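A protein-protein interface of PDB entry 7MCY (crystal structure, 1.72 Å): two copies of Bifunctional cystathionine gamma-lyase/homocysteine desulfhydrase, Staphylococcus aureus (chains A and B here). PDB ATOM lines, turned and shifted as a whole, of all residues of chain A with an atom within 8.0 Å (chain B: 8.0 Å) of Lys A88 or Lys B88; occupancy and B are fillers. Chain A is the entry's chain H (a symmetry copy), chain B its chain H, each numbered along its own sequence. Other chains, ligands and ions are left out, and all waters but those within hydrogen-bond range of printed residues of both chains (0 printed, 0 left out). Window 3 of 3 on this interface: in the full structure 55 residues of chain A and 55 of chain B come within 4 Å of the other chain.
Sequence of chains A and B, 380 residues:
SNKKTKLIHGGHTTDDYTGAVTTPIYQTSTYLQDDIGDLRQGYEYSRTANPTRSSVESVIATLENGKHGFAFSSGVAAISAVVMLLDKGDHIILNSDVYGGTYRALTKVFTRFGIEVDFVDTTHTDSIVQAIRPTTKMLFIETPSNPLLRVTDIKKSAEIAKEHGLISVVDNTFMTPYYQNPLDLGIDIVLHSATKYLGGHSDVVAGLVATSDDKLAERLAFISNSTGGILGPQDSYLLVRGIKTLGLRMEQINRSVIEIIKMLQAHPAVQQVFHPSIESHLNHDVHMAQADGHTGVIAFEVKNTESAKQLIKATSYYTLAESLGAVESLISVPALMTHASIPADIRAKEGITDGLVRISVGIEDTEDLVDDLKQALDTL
NH2 of Arg A112 lies within hydrogen-bond range of O of Met B84 (2.9 Å).
NH1 of Arg A112 lies within hydrogen-bond range of O of Leu B86 (2.9 Å).
OD1 of Asp B87 is in salt-bridge range of NH1 of Arg A112 (3.0 Å).
N of Lys B88 is in hydrogen-bond range of O of Arg A112 (2.9 Å).
The backbone carbonyl oxygen (O) of Met A84 lies within hydrogen-bond range of the guanidinium group (NH2) of Arg B112.
NH1 of Arg B112 sits at hydrogen-bond distance from O of Leu A86 (2.9 Å).
The guanidinium group (NH1) of Arg B112 is in salt-bridge range of the side-chain carboxylate (OD1) of Asp A87.
O of Arg B112 lies within hydrogen-bond range of N of Lys A88 (2.9 Å).
The side-chain carboxylate (OD2) of Asp B90 lies within hydrogen-bond range of the backbone NH (N) of Asp B87 (2.9 Å).
N of Gly B89 lies within hydrogen-bond range of O of Gly B114.
The side-chain carboxylate of Asp A90 lies within hydrogen-bond range of the backbone NH of Asp A87, 2.9 Å away.
The backbone NH (N) of Gly A89 is in hydrogen-bond range of the backbone carbonyl oxygen (O) of Gly A114 (2.8 Å).
Among the printed residues, merely in contact across the chains: Leu A86 with Phe B113, Phe A113 with Leu B86, Met A84 with Met B84, Phe A113 with Phe B113, Lys A88 with Lys B88, Met A84 with Phe B113, Phe A113 with Met B84, Lys A88 with Gly B114 and Gly A114 with Lys B88.
Of chain B, only Lys B88 (3.6 Å), Arg B112 (2.9 Å) and Gly B114 (3.9 Å) come within 4 Å of Lys A88.
Of the printed residues of chain A, Lys B88 touches Lys A88, Arg A112 and Gly A114.
Printed residues of chain A within 4 Å of Phe B113: Met A84, Leu A86 and Phe A113.
Printed residues of chain A within 4 Å of Leu B86: Arg A112 (2.9 Å) and Phe A113 (3.1 Å).
Of the printed residues of chain B, Met A84 touches Met B84 (3.3 Å), Arg B112 (2.9 Å) and Phe B113 (3.6 Å).
Printed residues of chain B within 4 Å of Leu A86: Arg B112 and Phe B113.
Phe B110 touches none of the printed residues of chain A.
The nearest printed residue of chain A that does not touch Asp B87 is Phe A113 (4.5 Å).
Of the 18 printed residues of chain A, 7 touch a printed residue of chain B.
Hydrophobic or aromatic side chains of chain A within 4 Å of the printed part of chain B: Met A84 and Phe A113.
Of the 18 printed residues of chain B, 7 touch a printed residue of chain A.
Met A84 touches Arg B112, and with the chains exchanged Arg A112 touches Met B84.
Met A84 touches Phe B113, and with the chains exchanged Phe A113 touches Met B84.
Leu A86 touches Phe B113, and with the chains exchanged Phe A113 touches Leu B86.
Phe B113 touches its own counterpart, Phe A113.
18 positions are printed for both chains.
Of the 17 pairs that touch across the chains among the printed residues, 17 have their exchanged pair printed and touching as well.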
ATOM      1  N   VAL A  83       4.851 -17.950  -6.624  1.00  0.00           N
ATOM      2  CA  VAL A  83       6.267 -17.559  -6.696  1.00  0.00           C
ATOM      3  C   VAL A  83       6.513 -16.660  -7.900  1.00  0.00           C
ATOM      4  O   VAL A  83       7.350 -15.747  -7.849  1.00  0.00           O
ATOM      5  CB  VAL A  83       7.185 -18.802  -6.733  1.00  0.00           C
ATOM      6  CG1 VAL A  83       8.653 -18.397  -7.029  1.00  0.00           C
ATOM      7  CG2 VAL A  83       7.109 -19.560  -5.417  1.00  0.00           C
ATOM      8  N   MET A  84       5.788 -16.888  -8.996  1.00  0.00           N
ATOM      9  CA  MET A  84       5.972 -16.067 -10.187  1.00  0.00           C
ATOM     10  C   MET A  84       5.477 -14.634 -10.030  1.00  0.00           C
ATOM     11  O   MET A  84       5.651 -13.841 -10.967  1.00  0.00           O
ATOM     12  CB  MET A  84       5.278 -16.727 -11.373  1.00  0.00           C
ATOM     13  CG  MET A  84       6.091 -17.867 -11.958  1.00  0.00           C
ATOM     14  SD  MET A  84       5.235 -18.552 -13.375  1.00  0.00           S
ATOM     15  CE  MET A  84       6.576 -19.347 -14.176  1.00  0.00           C
ATOM     16  N   LEU A  85       4.851 -14.285  -8.904  1.00  0.00           N
ATOM     17  CA  LEU A  85       4.613 -12.882  -8.591  1.00  0.00           C
ATOM     18  C   LEU A  85       5.917 -12.100  -8.476  1.00  0.00           C
ATOM     19  O   LEU A  85       5.909 -10.877  -8.644  1.00  0.00           O
ATOM     20  CB  LEU A  85       3.833 -12.756  -7.286  1.00  0.00           C
ATOM     21  CG  LEU A  85       2.389 -13.286  -7.325  1.00  0.00           C
ATOM     22  CD1 LEU A  85       1.846 -13.374  -5.916  1.00  0.00           C
ATOM     23  CD2 LEU A  85       1.528 -12.376  -8.173  1.00  0.00           C
ATOM     24  N   LEU A  86       7.025 -12.782  -8.214  1.00  0.00           N
ATOM     25  CA  LEU A  86       8.317 -12.146  -7.975  1.00  0.00           C
ATOM     26  C   LEU A  86       9.163 -12.101  -9.247  1.00  0.00           C
ATOM     27  O   LEU A  86       8.886 -12.780 -10.235  1.00  0.00           O
ATOM     28  CB  LEU A  86       9.061 -12.898  -6.871  1.00  0.00           C
ATOM     29  CG  LEU A  86       8.302 -13.025  -5.551  1.00  0.00           C
ATOM     30  CD1 LEU A  86       9.174 -13.723  -4.537  1.00  0.00           C
ATOM     31  CD2 LEU A  86       7.817 -11.679  -5.015  1.00  0.00           C
ATOM     32  N   ASP A  87      10.236 -11.299  -9.195  1.00  0.00           N
ATOM     33  CA  ASP A  87      11.196 -11.132 -10.280  1.00  0.00           C
ATOM     34  C   ASP A  87      12.555 -11.699  -9.888  1.00  0.00           C
ATOM     35  O   ASP A  87      12.871 -11.849  -8.706  1.00  0.00           O
ATOM     36  CB  ASP A  87      11.418  -9.648 -10.627  1.00  0.00           C
ATOM     37  CG  ASP A  87      10.166  -8.941 -11.084  1.00  0.00           C
ATOM     38  OD1 ASP A  87       9.157  -9.600 -11.399  1.00  0.00           O
ATOM     39  OD2 ASP A  87      10.198  -7.698 -11.128  1.00  0.00           O
ATOM     40  N   LYS A  88      13.378 -11.965 -10.900  1.00  0.00           N
ATOM     41  CA  LYS A  88      14.787 -12.248 -10.674  1.00  0.00           C
ATOM     42  C   LYS A  88      15.379 -11.203  -9.733  1.00  0.00           C
ATOM     43  O   LYS A  88      15.084 -10.010  -9.849  1.00  0.00           O
ATOM     44  CB  LYS A  88      15.522 -12.255 -12.014  1.00  0.00           C
ATOM     45  CG  LYS A  88      17.033 -12.138 -11.939  1.00  0.00           C
ATOM     46  CD  LYS A  88      17.577 -11.409 -13.169  1.00  0.00           C
ATOM     47  CE  LYS A  88      16.507 -10.551 -13.844  1.00  0.00           C
ATOM     48  N   GLY A  89      16.161 -11.665  -8.756  1.00  0.00           N
ATOM     49  CA  GLY A  89      16.737 -10.795  -7.750  1.00  0.00           C
ATOM     50  C   GLY A  89      15.923 -10.656  -6.476  1.00  0.00           C
ATOM     51  O   GLY A  89      16.465 -10.213  -5.457  1.00  0.00           O
ATOM     52  N   ASP A  90      14.642 -11.018  -6.498  1.00  0.00           N
ATOM     53  CA  ASP A  90      13.821 -10.977  -5.298  1.00  0.00           C
ATOM     54  C   ASP A  90      14.127 -12.180  -4.398  1.00  0.00           C
ATOM     55  O   ASP A  90      14.567 -13.239  -4.854  1.00  0.00           O
ATOM     56  CB  ASP A  90      12.325 -10.989  -5.658  1.00  0.00           C
ATOM     57  CG  ASP A  90      11.856  -9.696  -6.310  1.00  0.00           C
ATOM     58  OD1 ASP A  90      12.606  -8.678  -6.298  1.00  0.00           O
ATOM     59  OD2 ASP A  90      10.717  -9.698  -6.828  1.00  0.00           O
ATOM     60  N   HIS A  91      13.832 -12.020  -3.112  1.00  0.00           N
ATOM     61  CA  HIS A  91      14.157 -13.012  -2.095  1.00  0.00           C
ATOM     62  C   HIS A  91      12.898 -13.438  -1.342  1.00  0.00           C
ATOM     63  O   HIS A  91      12.003 -12.615  -1.093  1.00  0.00           O
ATOM     64  CB  HIS A  91      15.227 -12.417  -1.147  1.00  0.00           C
ATOM     65  CG  HIS A  91      15.590 -13.283   0.020  1.00  0.00           C
ATOM     66  ND1 HIS A  91      15.139 -13.029   1.297  1.00  0.00           N
ATOM     67  CD2 HIS A  91      16.431 -14.342   0.122  1.00  0.00           C
ATOM     68  CE1 HIS A  91      15.652 -13.917   2.131  1.00  0.00           C
ATOM     69  NE2 HIS A  91      16.441 -14.725   1.444  1.00  0.00           N
ATOM     70  N   VAL A 109      14.257 -25.179  -9.558  1.00  0.00           N
ATOM     71  CA  VAL A 109      13.660 -24.455 -10.678  1.00  0.00           C
ATOM     72  C   VAL A 109      13.817 -22.941 -10.503  1.00  0.00           C
ATOM     73  O   VAL A 109      14.515 -22.288 -11.276  1.00  0.00           O
ATOM     74  CB  VAL A 109      12.181 -24.854 -10.891  1.00  0.00           C
ATOM     75  CG1 VAL A 109      11.605 -24.106 -12.088  1.00  0.00           C
ATOM     76  CG2 VAL A 109      12.056 -26.358 -11.108  1.00  0.00           C
ATOM     77  N   PHE A 110      13.212 -22.375  -9.458  1.00  0.00           N
ATOM     78  CA  PHE A 110      13.127 -20.919  -9.417  1.00  0.00           C
ATOM     79  C   PHE A 110      14.453 -20.245  -9.099  1.00  0.00           C
ATOM     80  O   PHE A 110      14.645 -19.098  -9.511  1.00  0.00           O
ATOM     81  CB  PHE A 110      12.036 -20.493  -8.448  1.00  0.00           C
ATOM     82  CG  PHE A 110      10.671 -20.804  -8.984  1.00  0.00           C
ATOM     83  CD1 PHE A 110      10.177 -20.091 -10.069  1.00  0.00           C
ATOM     84  CD2 PHE A 110       9.937 -21.862  -8.488  1.00  0.00           C
ATOM     85  CE1 PHE A 110       8.940 -20.391 -10.617  1.00  0.00           C
ATOM     86  CE2 PHE A 110       8.694 -22.172  -9.036  1.00  0.00           C
ATOM     87  CZ  PHE A 110       8.201 -21.437 -10.100  1.00  0.00           C
ATOM     88  N   THR A 111      15.386 -20.929  -8.429  1.00  0.00           N
ATOM     89  CA  THR A 111      16.706 -20.310  -8.271  1.00  0.00           C
ATOM     90  C   THR A 111      17.417 -20.165  -9.611  1.00  0.00           C
ATOM     91  O   THR A 111      18.283 -19.292  -9.758  1.00  0.00           O
ATOM     92  CB  THR A 111      17.588 -21.103  -7.306  1.00  0.00           C
ATOM     93  OG1 THR A 111      17.645 -22.473  -7.724  1.00  0.00           O
ATOM     94  CG2 THR A 111      17.048 -21.006  -5.879  1.00  0.00           C
ATOM     95  N   ARG A 112      17.082 -21.002 -10.597  1.00  0.00           N
ATOM     96  CA  ARG A 112      17.653 -20.818 -11.927  1.00  0.00           C
ATOM     97  C   ARG A 112      17.148 -19.545 -12.586  1.00  0.00           C
ATOM     98  O   ARG A 112      17.771 -19.062 -13.539  1.00  0.00           O
ATOM     99  CB  ARG A 112      17.355 -22.026 -12.814  1.00  0.00           C
ATOM    100  CG  ARG A 112      17.955 -23.315 -12.298  1.00  0.00           C
ATOM    101  CD  ARG A 112      17.880 -24.423 -13.327  1.00  0.00           C
ATOM    102  NE  ARG A 112      16.523 -24.955 -13.493  1.00  0.00           N
ATOM    103  CZ  ARG A 112      15.706 -24.642 -14.495  1.00  0.00           C
ATOM    104  NH1 ARG A 112      16.096 -23.780 -15.428  1.00  0.00           N
ATOM    105  NH2 ARG A 112      14.490 -25.197 -14.566  1.00  0.00           N
ATOM    106  N   PHE A 113      16.049 -18.982 -12.088  1.00  0.00           N
ATOM    107  CA  PHE A 113      15.506 -17.735 -12.597  1.00  0.00           C
ATOM    108  C   PHE A 113      15.860 -16.551 -11.710  1.00  0.00           C
ATOM    109  O   PHE A 113      15.246 -15.488 -11.834  1.00  0.00           O
ATOM    110  CB  PHE A 113      13.994 -17.858 -12.763  1.00  0.00           C
ATOM    111  CG  PHE A 113      13.593 -19.008 -13.645  1.00  0.00           C
ATOM    112  CD1 PHE A 113      14.148 -19.148 -14.906  1.00  0.00           C
ATOM    113  CD2 PHE A 113      12.707 -19.964 -13.203  1.00  0.00           C
ATOM    114  CE1 PHE A 113      13.806 -20.208 -15.718  1.00  0.00           C
ATOM    115  CE2 PHE A 113      12.366 -21.029 -14.010  1.00  0.00           C
ATOM    116  CZ  PHE A 113      12.928 -21.150 -15.269  1.00  0.00           C
ATOM    117  N   GLY A 114      16.836 -16.712 -10.821  1.00  0.00           N
ATOM    118  CA  GLY A 114      17.291 -15.602 -10.015  1.00  0.00           C
ATOM    119  C   GLY A 114      16.474 -15.314  -8.778  1.00  0.00           C
ATOM    120  O   GLY A 114      16.728 -14.301  -8.120  1.00  0.00           O
ATOM    121  N   ILE A 115      15.495 -16.151  -8.448  1.00  0.00           N
ATOM    122  CA  ILE A 115      14.799 -16.030  -7.172  1.00  0.00           C
ATOM    123  C   ILE A 115      15.711 -16.568  -6.078  1.00  0.00           C
ATOM    124  O   ILE A 115      16.246 -17.675  -6.196  1.00  0.00           O
ATOM    125  CB  ILE A 115      13.468 -16.798  -7.197  1.00  0.00           C
ATOM    126  CG1 ILE A 115      12.583 -16.321  -8.352  1.00  0.00           C
ATOM    127  CG2 ILE A 115      12.740 -16.641  -5.867  1.00  0.00           C
ATOM    128  CD1 ILE A 115      12.217 -14.877  -8.260  1.00  0.00           C
ATOM    129  N   GLU A 116      15.880 -15.801  -5.008  1.00  0.00           N
ATOM    130  CA  GLU A 116      16.700 -16.225  -3.876  1.00  0.00           C
ATOM    131  C   GLU A 116      15.810 -16.667  -2.723  1.00  0.00           C
ATOM    132  O   GLU A 116      14.746 -16.082  -2.486  1.00  0.00           O
ATOM    133  CB  GLU A 116      17.621 -15.093  -3.420  1.00  0.00           C
ATOM    134  CG  GLU A 116      18.468 -14.496  -4.529  1.00  0.00           C
ATOM    135  CD  GLU A 116      19.661 -15.366  -4.888  1.00  0.00           C
ATOM    136  OE1 GLU A 116      19.842 -16.427  -4.251  1.00  0.00           O
ATOM    137  OE2 GLU A 116      20.434 -14.973  -5.789  1.00  0.00           O
ATOM    138  N   THR A 135      16.342  -7.189  -0.380  1.00  0.00           N
ATOM    139  CA  THR A 135      15.675  -7.745  -1.550  1.00  0.00           C
ATOM    140  C   THR A 135      14.495  -8.650  -1.209  1.00  0.00           C
ATOM    141  O   THR A 135      13.827  -9.125  -2.131  1.00  0.00           O
ATOM    142  CB  THR A 135      16.678  -8.537  -2.387  1.00  0.00           C
ATOM    143  OG1 THR A 135      17.331  -9.491  -1.540  1.00  0.00           O
ATOM    144  CG2 THR A 135      17.731  -7.593  -3.002  1.00  0.00           C
ATOM    145  N   VAL B  83      10.122 -23.450 -21.986  1.00  0.00           N
ATOM    146  CA  VAL B  83      10.949 -22.267 -21.709  1.00  0.00           C
ATOM    147  C   VAL B  83      11.724 -22.448 -20.410  1.00  0.00           C
ATOM    148  O   VAL B  83      12.862 -21.975 -20.280  1.00  0.00           O
ATOM    149  CB  VAL B  83      10.086 -20.984 -21.667  1.00  0.00           C
ATOM    150  CG1 VAL B  83      10.917 -19.776 -21.160  1.00  0.00           C
ATOM    151  CG2 VAL B  83       9.514 -20.682 -23.042  1.00  0.00           C
ATOM    152  N   MET B  84      11.136 -23.142 -19.435  1.00  0.00           N
ATOM    153  CA  MET B  84      11.820 -23.354 -18.165  1.00  0.00           C
ATOM    154  C   MET B  84      13.015 -24.295 -18.258  1.00  0.00           C
ATOM    155  O   MET B  84      13.699 -24.485 -17.242  1.00  0.00           O
ATOM    156  CB  MET B  84      10.826 -23.879 -17.133  1.00  0.00           C
ATOM    157  CG  MET B  84       9.959 -22.777 -16.554  1.00  0.00           C
ATOM    158  SD  MET B  84       8.861 -23.464 -15.315  1.00  0.00           S
ATOM    159  CE  MET B  84       8.465 -22.005 -14.428  1.00  0.00           C
ATOM    160  N   LEU B  85      13.270 -24.904 -19.417  1.00  0.00           N
ATOM    161  CA  LEU B  85      14.542 -25.582 -19.636  1.00  0.00           C
ATOM    162  C   LEU B  85      15.721 -24.621 -19.523  1.00  0.00           C
ATOM    163  O   LEU B  85      16.841 -25.063 -19.253  1.00  0.00           O
ATOM    164  CB  LEU B  85      14.561 -26.243 -21.011  1.00  0.00           C
ATOM    165  CG  LEU B  85      13.580 -27.415 -21.194  1.00  0.00           C
ATOM    166  CD1 LEU B  85      13.489 -27.771 -22.661  1.00  0.00           C
ATOM    167  CD2 LEU B  85      14.042 -28.605 -20.382  1.00  0.00           C
ATOM    168  N   LEU B  86      15.483 -23.328 -19.705  1.00  0.00           N
ATOM    169  CA  LEU B  86      16.536 -22.318 -19.729  1.00  0.00           C
ATOM    170  C   LEU B  86      16.704 -21.651 -18.364  1.00  0.00           C
ATOM    171  O   LEU B  86      15.856 -21.762 -17.480  1.00  0.00           O
ATOM    172  CB  LEU B  86      16.215 -21.269 -20.794  1.00  0.00           C
ATOM    173  CG  LEU B  86      16.005 -21.822 -22.204  1.00  0.00           C
ATOM    174  CD1 LEU B  86      15.766 -20.680 -23.159  1.00  0.00           C
ATOM    175  CD2 LEU B  86      17.168 -22.692 -22.677  1.00  0.00           C
ATOM    176  N   ASP B  87      17.816 -20.919 -18.215  1.00  0.00           N
ATOM    177  CA  ASP B  87      18.159 -20.171 -17.011  1.00  0.00           C
ATOM    178  C   ASP B  87      18.128 -18.671 -17.282  1.00  0.00           C
ATOM    179  O   ASP B  87      18.237 -18.223 -18.424  1.00  0.00           O
ATOM    180  CB  ASP B  87      19.579 -20.503 -16.513  1.00  0.00           C
ATOM    181  CG  ASP B  87      19.768 -21.956 -16.154  1.00  0.00           C
ATOM    182  OD1 ASP B  87      18.778 -22.700 -16.022  1.00  0.00           O
ATOM    183  OD2 ASP B  87      20.936 -22.357 -16.000  1.00  0.00           O
ATOM    184  N   LYS B  88      18.029 -17.898 -16.203  1.00  0.00           N
ATOM    185  CA  LYS B  88      18.260 -16.463 -16.279  1.00  0.00           C
ATOM    186  C   LYS B  88      19.549 -16.188 -17.047  1.00  0.00           C
ATOM    187  O   LYS B  88      20.552 -16.883 -16.866  1.00  0.00           O
ATOM    188  CB  LYS B  88      18.335 -15.888 -14.864  1.00  0.00           C
ATOM    189  CG  LYS B  88      18.954 -14.509 -14.743  1.00  0.00           C
ATOM    190  CD  LYS B  88      19.667 -14.355 -13.399  1.00  0.00           C
ATOM    191  CE  LYS B  88      20.032 -15.709 -12.788  1.00  0.00           C
ATOM    192  N   GLY B  89      19.496 -15.214 -17.957  1.00  0.00           N
ATOM    193  CA  GLY B  89      20.625 -14.888 -18.807  1.00  0.00           C
ATOM    194  C   GLY B  89      20.640 -15.587 -20.154  1.00  0.00           C
ATOM    195  O   GLY B  89      21.358 -15.145 -21.057  1.00  0.00           O
ATOM    196  N   ASP B  90      19.873 -16.663 -20.320  1.00  0.00           N
ATOM    197  CA  ASP B  90      19.785 -17.342 -21.604  1.00  0.00           C
ATOM    198  C   ASP B  90      18.872 -16.566 -22.559  1.00  0.00           C
ATOM    199  O   ASP B  90      17.971 -15.829 -22.145  1.00  0.00           O
ATOM    200  CB  ASP B  90      19.232 -18.768 -21.431  1.00  0.00           C
ATOM    201  CG  ASP B  90      20.207 -19.706 -20.733  1.00  0.00           C
ATOM    202  OD1 ASP B  90      21.409 -19.353 -20.566  1.00  0.00           O
ATOM    203  OD2 ASP B  90      19.763 -20.815 -20.360  1.00  0.00           O
ATOM    204  N   HIS B  91      19.080 -16.786 -23.852  1.00  0.00           N
ATOM    205  CA  HIS B  91      18.385 -16.054 -24.904  1.00  0.00           C
ATOM    206  C   HIS B  91      17.660 -17.021 -25.838  1.00  0.00           C
ATOM    207  O   HIS B  91      18.163 -18.119 -26.124  1.00  0.00           O
ATOM    208  CB  HIS B  91      19.412 -15.176 -25.659  1.00  0.00           C
ATOM    209  CG  HIS B  91      18.866 -14.439 -26.843  1.00  0.00           C
ATOM    210  ND1 HIS B  91      19.110 -14.839 -28.139  1.00  0.00           N
ATOM    211  CD2 HIS B  91      18.167 -13.280 -26.932  1.00  0.00           C
ATOM    212  CE1 HIS B  91      18.551 -13.982 -28.977  1.00  0.00           C
ATOM    213  NE2 HIS B  91      17.974 -13.026 -28.271  1.00  0.00           N
ATOM    214  N   VAL B 109       6.127 -12.422 -18.556  1.00  0.00           N
ATOM    215  CA  VAL B 109       6.469 -13.325 -17.459  1.00  0.00           C
ATOM    216  C   VAL B 109       7.958 -13.683 -17.483  1.00  0.00           C
ATOM    217  O   VAL B 109       8.706 -13.321 -16.577  1.00  0.00           O
ATOM    218  CB  VAL B 109       5.578 -14.590 -17.464  1.00  0.00           C
ATOM    219  CG1 VAL B 109       5.940 -15.488 -16.286  1.00  0.00           C
ATOM    220  CG2 VAL B 109       4.104 -14.209 -17.394  1.00  0.00           C
ATOM    221  N   PHE B 110       8.414 -14.354 -18.542  1.00  0.00           N
ATOM    222  CA  PHE B 110       9.753 -14.930 -18.468  1.00  0.00           C
ATOM    223  C   PHE B 110      10.862 -13.894 -18.563  1.00  0.00           C
ATOM    224  O   PHE B 110      11.949 -14.143 -18.034  1.00  0.00           O
ATOM    225  CB  PHE B 110       9.907 -16.014 -19.523  1.00  0.00           C
ATOM    226  CG  PHE B 110       9.097 -17.229 -19.186  1.00  0.00           C
ATOM    227  CD1 PHE B 110       9.468 -18.030 -18.113  1.00  0.00           C
ATOM    228  CD2 PHE B 110       7.925 -17.510 -19.857  1.00  0.00           C
ATOM    229  CE1 PHE B 110       8.709 -19.130 -17.748  1.00  0.00           C
ATOM    230  CE2 PHE B 110       7.155 -18.613 -19.494  1.00  0.00           C
ATOM    231  CZ  PHE B 110       7.549 -19.418 -18.439  1.00  0.00           C
ATOM    232  N   THR B 111      10.614 -12.729 -19.170  1.00  0.00           N
ATOM    233  CA  THR B 111      11.651 -11.694 -19.111  1.00  0.00           C
ATOM    234  C   THR B 111      11.859 -11.193 -17.687  1.00  0.00           C
ATOM    235  O   THR B 111      12.946 -10.696 -17.362  1.00  0.00           O
ATOM    236  CB  THR B 111      11.320 -10.514 -20.026  1.00  0.00           C
ATOM    237  OG1 THR B 111      10.007 -10.026 -19.723  1.00  0.00           O
ATOM    238  CG2 THR B 111      11.406 -10.929 -21.495  1.00  0.00           C
ATOM    239  N   ARG B 112      10.845 -11.304 -16.825  1.00  0.00           N
ATOM    240  CA  ARG B 112      11.044 -10.947 -15.425  1.00  0.00           C
ATOM    241  C   ARG B 112      11.987 -11.913 -14.725  1.00  0.00           C
ATOM    242  O   ARG B 112      12.529 -11.578 -13.665  1.00  0.00           O
ATOM    243  CB  ARG B 112       9.707 -10.887 -14.687  1.00  0.00           C
ATOM    244  CG  ARG B 112       8.764  -9.839 -15.235  1.00  0.00           C
ATOM    245  CD  ARG B 112       7.577  -9.616 -14.321  1.00  0.00           C
ATOM    246  NE  ARG B 112       6.608 -10.718 -14.369  1.00  0.00           N
ATOM    247  CZ  ARG B 112       6.507 -11.675 -13.452  1.00  0.00           C
ATOM    248  NH1 ARG B 112       7.329 -11.686 -12.407  1.00  0.00           N
ATOM    249  NH2 ARG B 112       5.575 -12.627 -13.577  1.00  0.00           N
ATOM    250  N   PHE B 113      12.209 -13.091 -15.303  1.00  0.00           N
ATOM    251  CA  PHE B 113      13.133 -14.072 -14.760  1.00  0.00           C
ATOM    252  C   PHE B 113      14.466 -14.071 -15.492  1.00  0.00           C
ATOM    253  O   PHE B 113      15.241 -15.020 -15.353  1.00  0.00           O
ATOM    254  CB  PHE B 113      12.494 -15.457 -14.791  1.00  0.00           C
ATOM    255  CG  PHE B 113      11.178 -15.513 -14.066  1.00  0.00           C
ATOM    256  CD1 PHE B 113      11.078 -15.055 -12.764  1.00  0.00           C
ATOM    257  CD2 PHE B 113      10.044 -15.976 -14.693  1.00  0.00           C
ATOM    258  CE1 PHE B 113       9.873 -15.079 -12.094  1.00  0.00           C
ATOM    259  CE2 PHE B 113       8.836 -15.998 -14.029  1.00  0.00           C
ATOM    260  CZ  PHE B 113       8.755 -15.539 -12.726  1.00  0.00           C
ATOM    261  N   GLY B 114      14.747 -13.027 -16.265  1.00  0.00           N
ATOM    262  CA  GLY B 114      16.036 -12.913 -16.912  1.00  0.00           C
ATOM    263  C   GLY B 114      16.185 -13.669 -18.210  1.00  0.00           C
ATOM    264  O   GLY B 114      17.297 -13.724 -18.743  1.00  0.00           O
ATOM    265  N   ILE B 115      15.117 -14.270 -18.728  1.00  0.00           N
ATOM    266  CA  ILE B 115      15.155 -14.853 -20.064  1.00  0.00           C
ATOM    267  C   ILE B 115      15.089 -13.721 -21.080  1.00  0.00           C
ATOM    268  O   ILE B 115      14.216 -12.851 -20.993  1.00  0.00           O
ATOM    269  CB  ILE B 115      13.992 -15.836 -20.268  1.00  0.00           C
ATOM    270  CG1 ILE B 115      14.003 -16.926 -19.193  1.00  0.00           C
ATOM    271  CG2 ILE B 115      14.059 -16.457 -21.659  1.00  0.00           C
ATOM    272  CD1 ILE B 115      15.243 -17.757 -19.205  1.00  0.00           C
ATOM    273  N   GLU B 116      15.993 -13.734 -22.052  1.00  0.00           N
ATOM    274  CA  GLU B 116      16.007 -12.725 -23.107  1.00  0.00           C
ATOM    275  C   GLU B 116      15.439 -13.307 -24.394  1.00  0.00           C
ATOM    276  O   GLU B 116      15.661 -14.482 -24.708  1.00  0.00           O
ATOM    277  CB  GLU B 116      17.427 -12.213 -23.349  1.00  0.00           C
ATOM    278  CG  GLU B 116      18.131 -11.721 -22.098  1.00  0.00           C
ATOM    279  CD  GLU B 116      17.670 -10.338 -21.672  1.00  0.00           C
ATOM    280  OE1 GLU B 116      16.816  -9.749 -22.370  1.00  0.00           O
ATOM    281  OE2 GLU B 116      18.184  -9.827 -20.653  1.00  0.00           O
ATOM    282  N   THR B 135      24.766 -15.863 -25.833  1.00  0.00           N
ATOM    283  CA  THR B 135      23.882 -16.397 -24.806  1.00  0.00           C
ATOM    284  C   THR B 135      22.685 -17.160 -25.365  1.00  0.00           C
ATOM    285  O   THR B 135      21.906 -17.701 -24.575  1.00  0.00           O
ATOM    286  CB  THR B 135      23.372 -15.258 -23.923  1.00  0.00           C
ATOM    287  OG1 THR B 135      22.800 -14.247 -24.763  1.00  0.00           O
ATOM    288  CG2 THR B 135      24.529 -14.650 -23.105  1.00  0.00           C
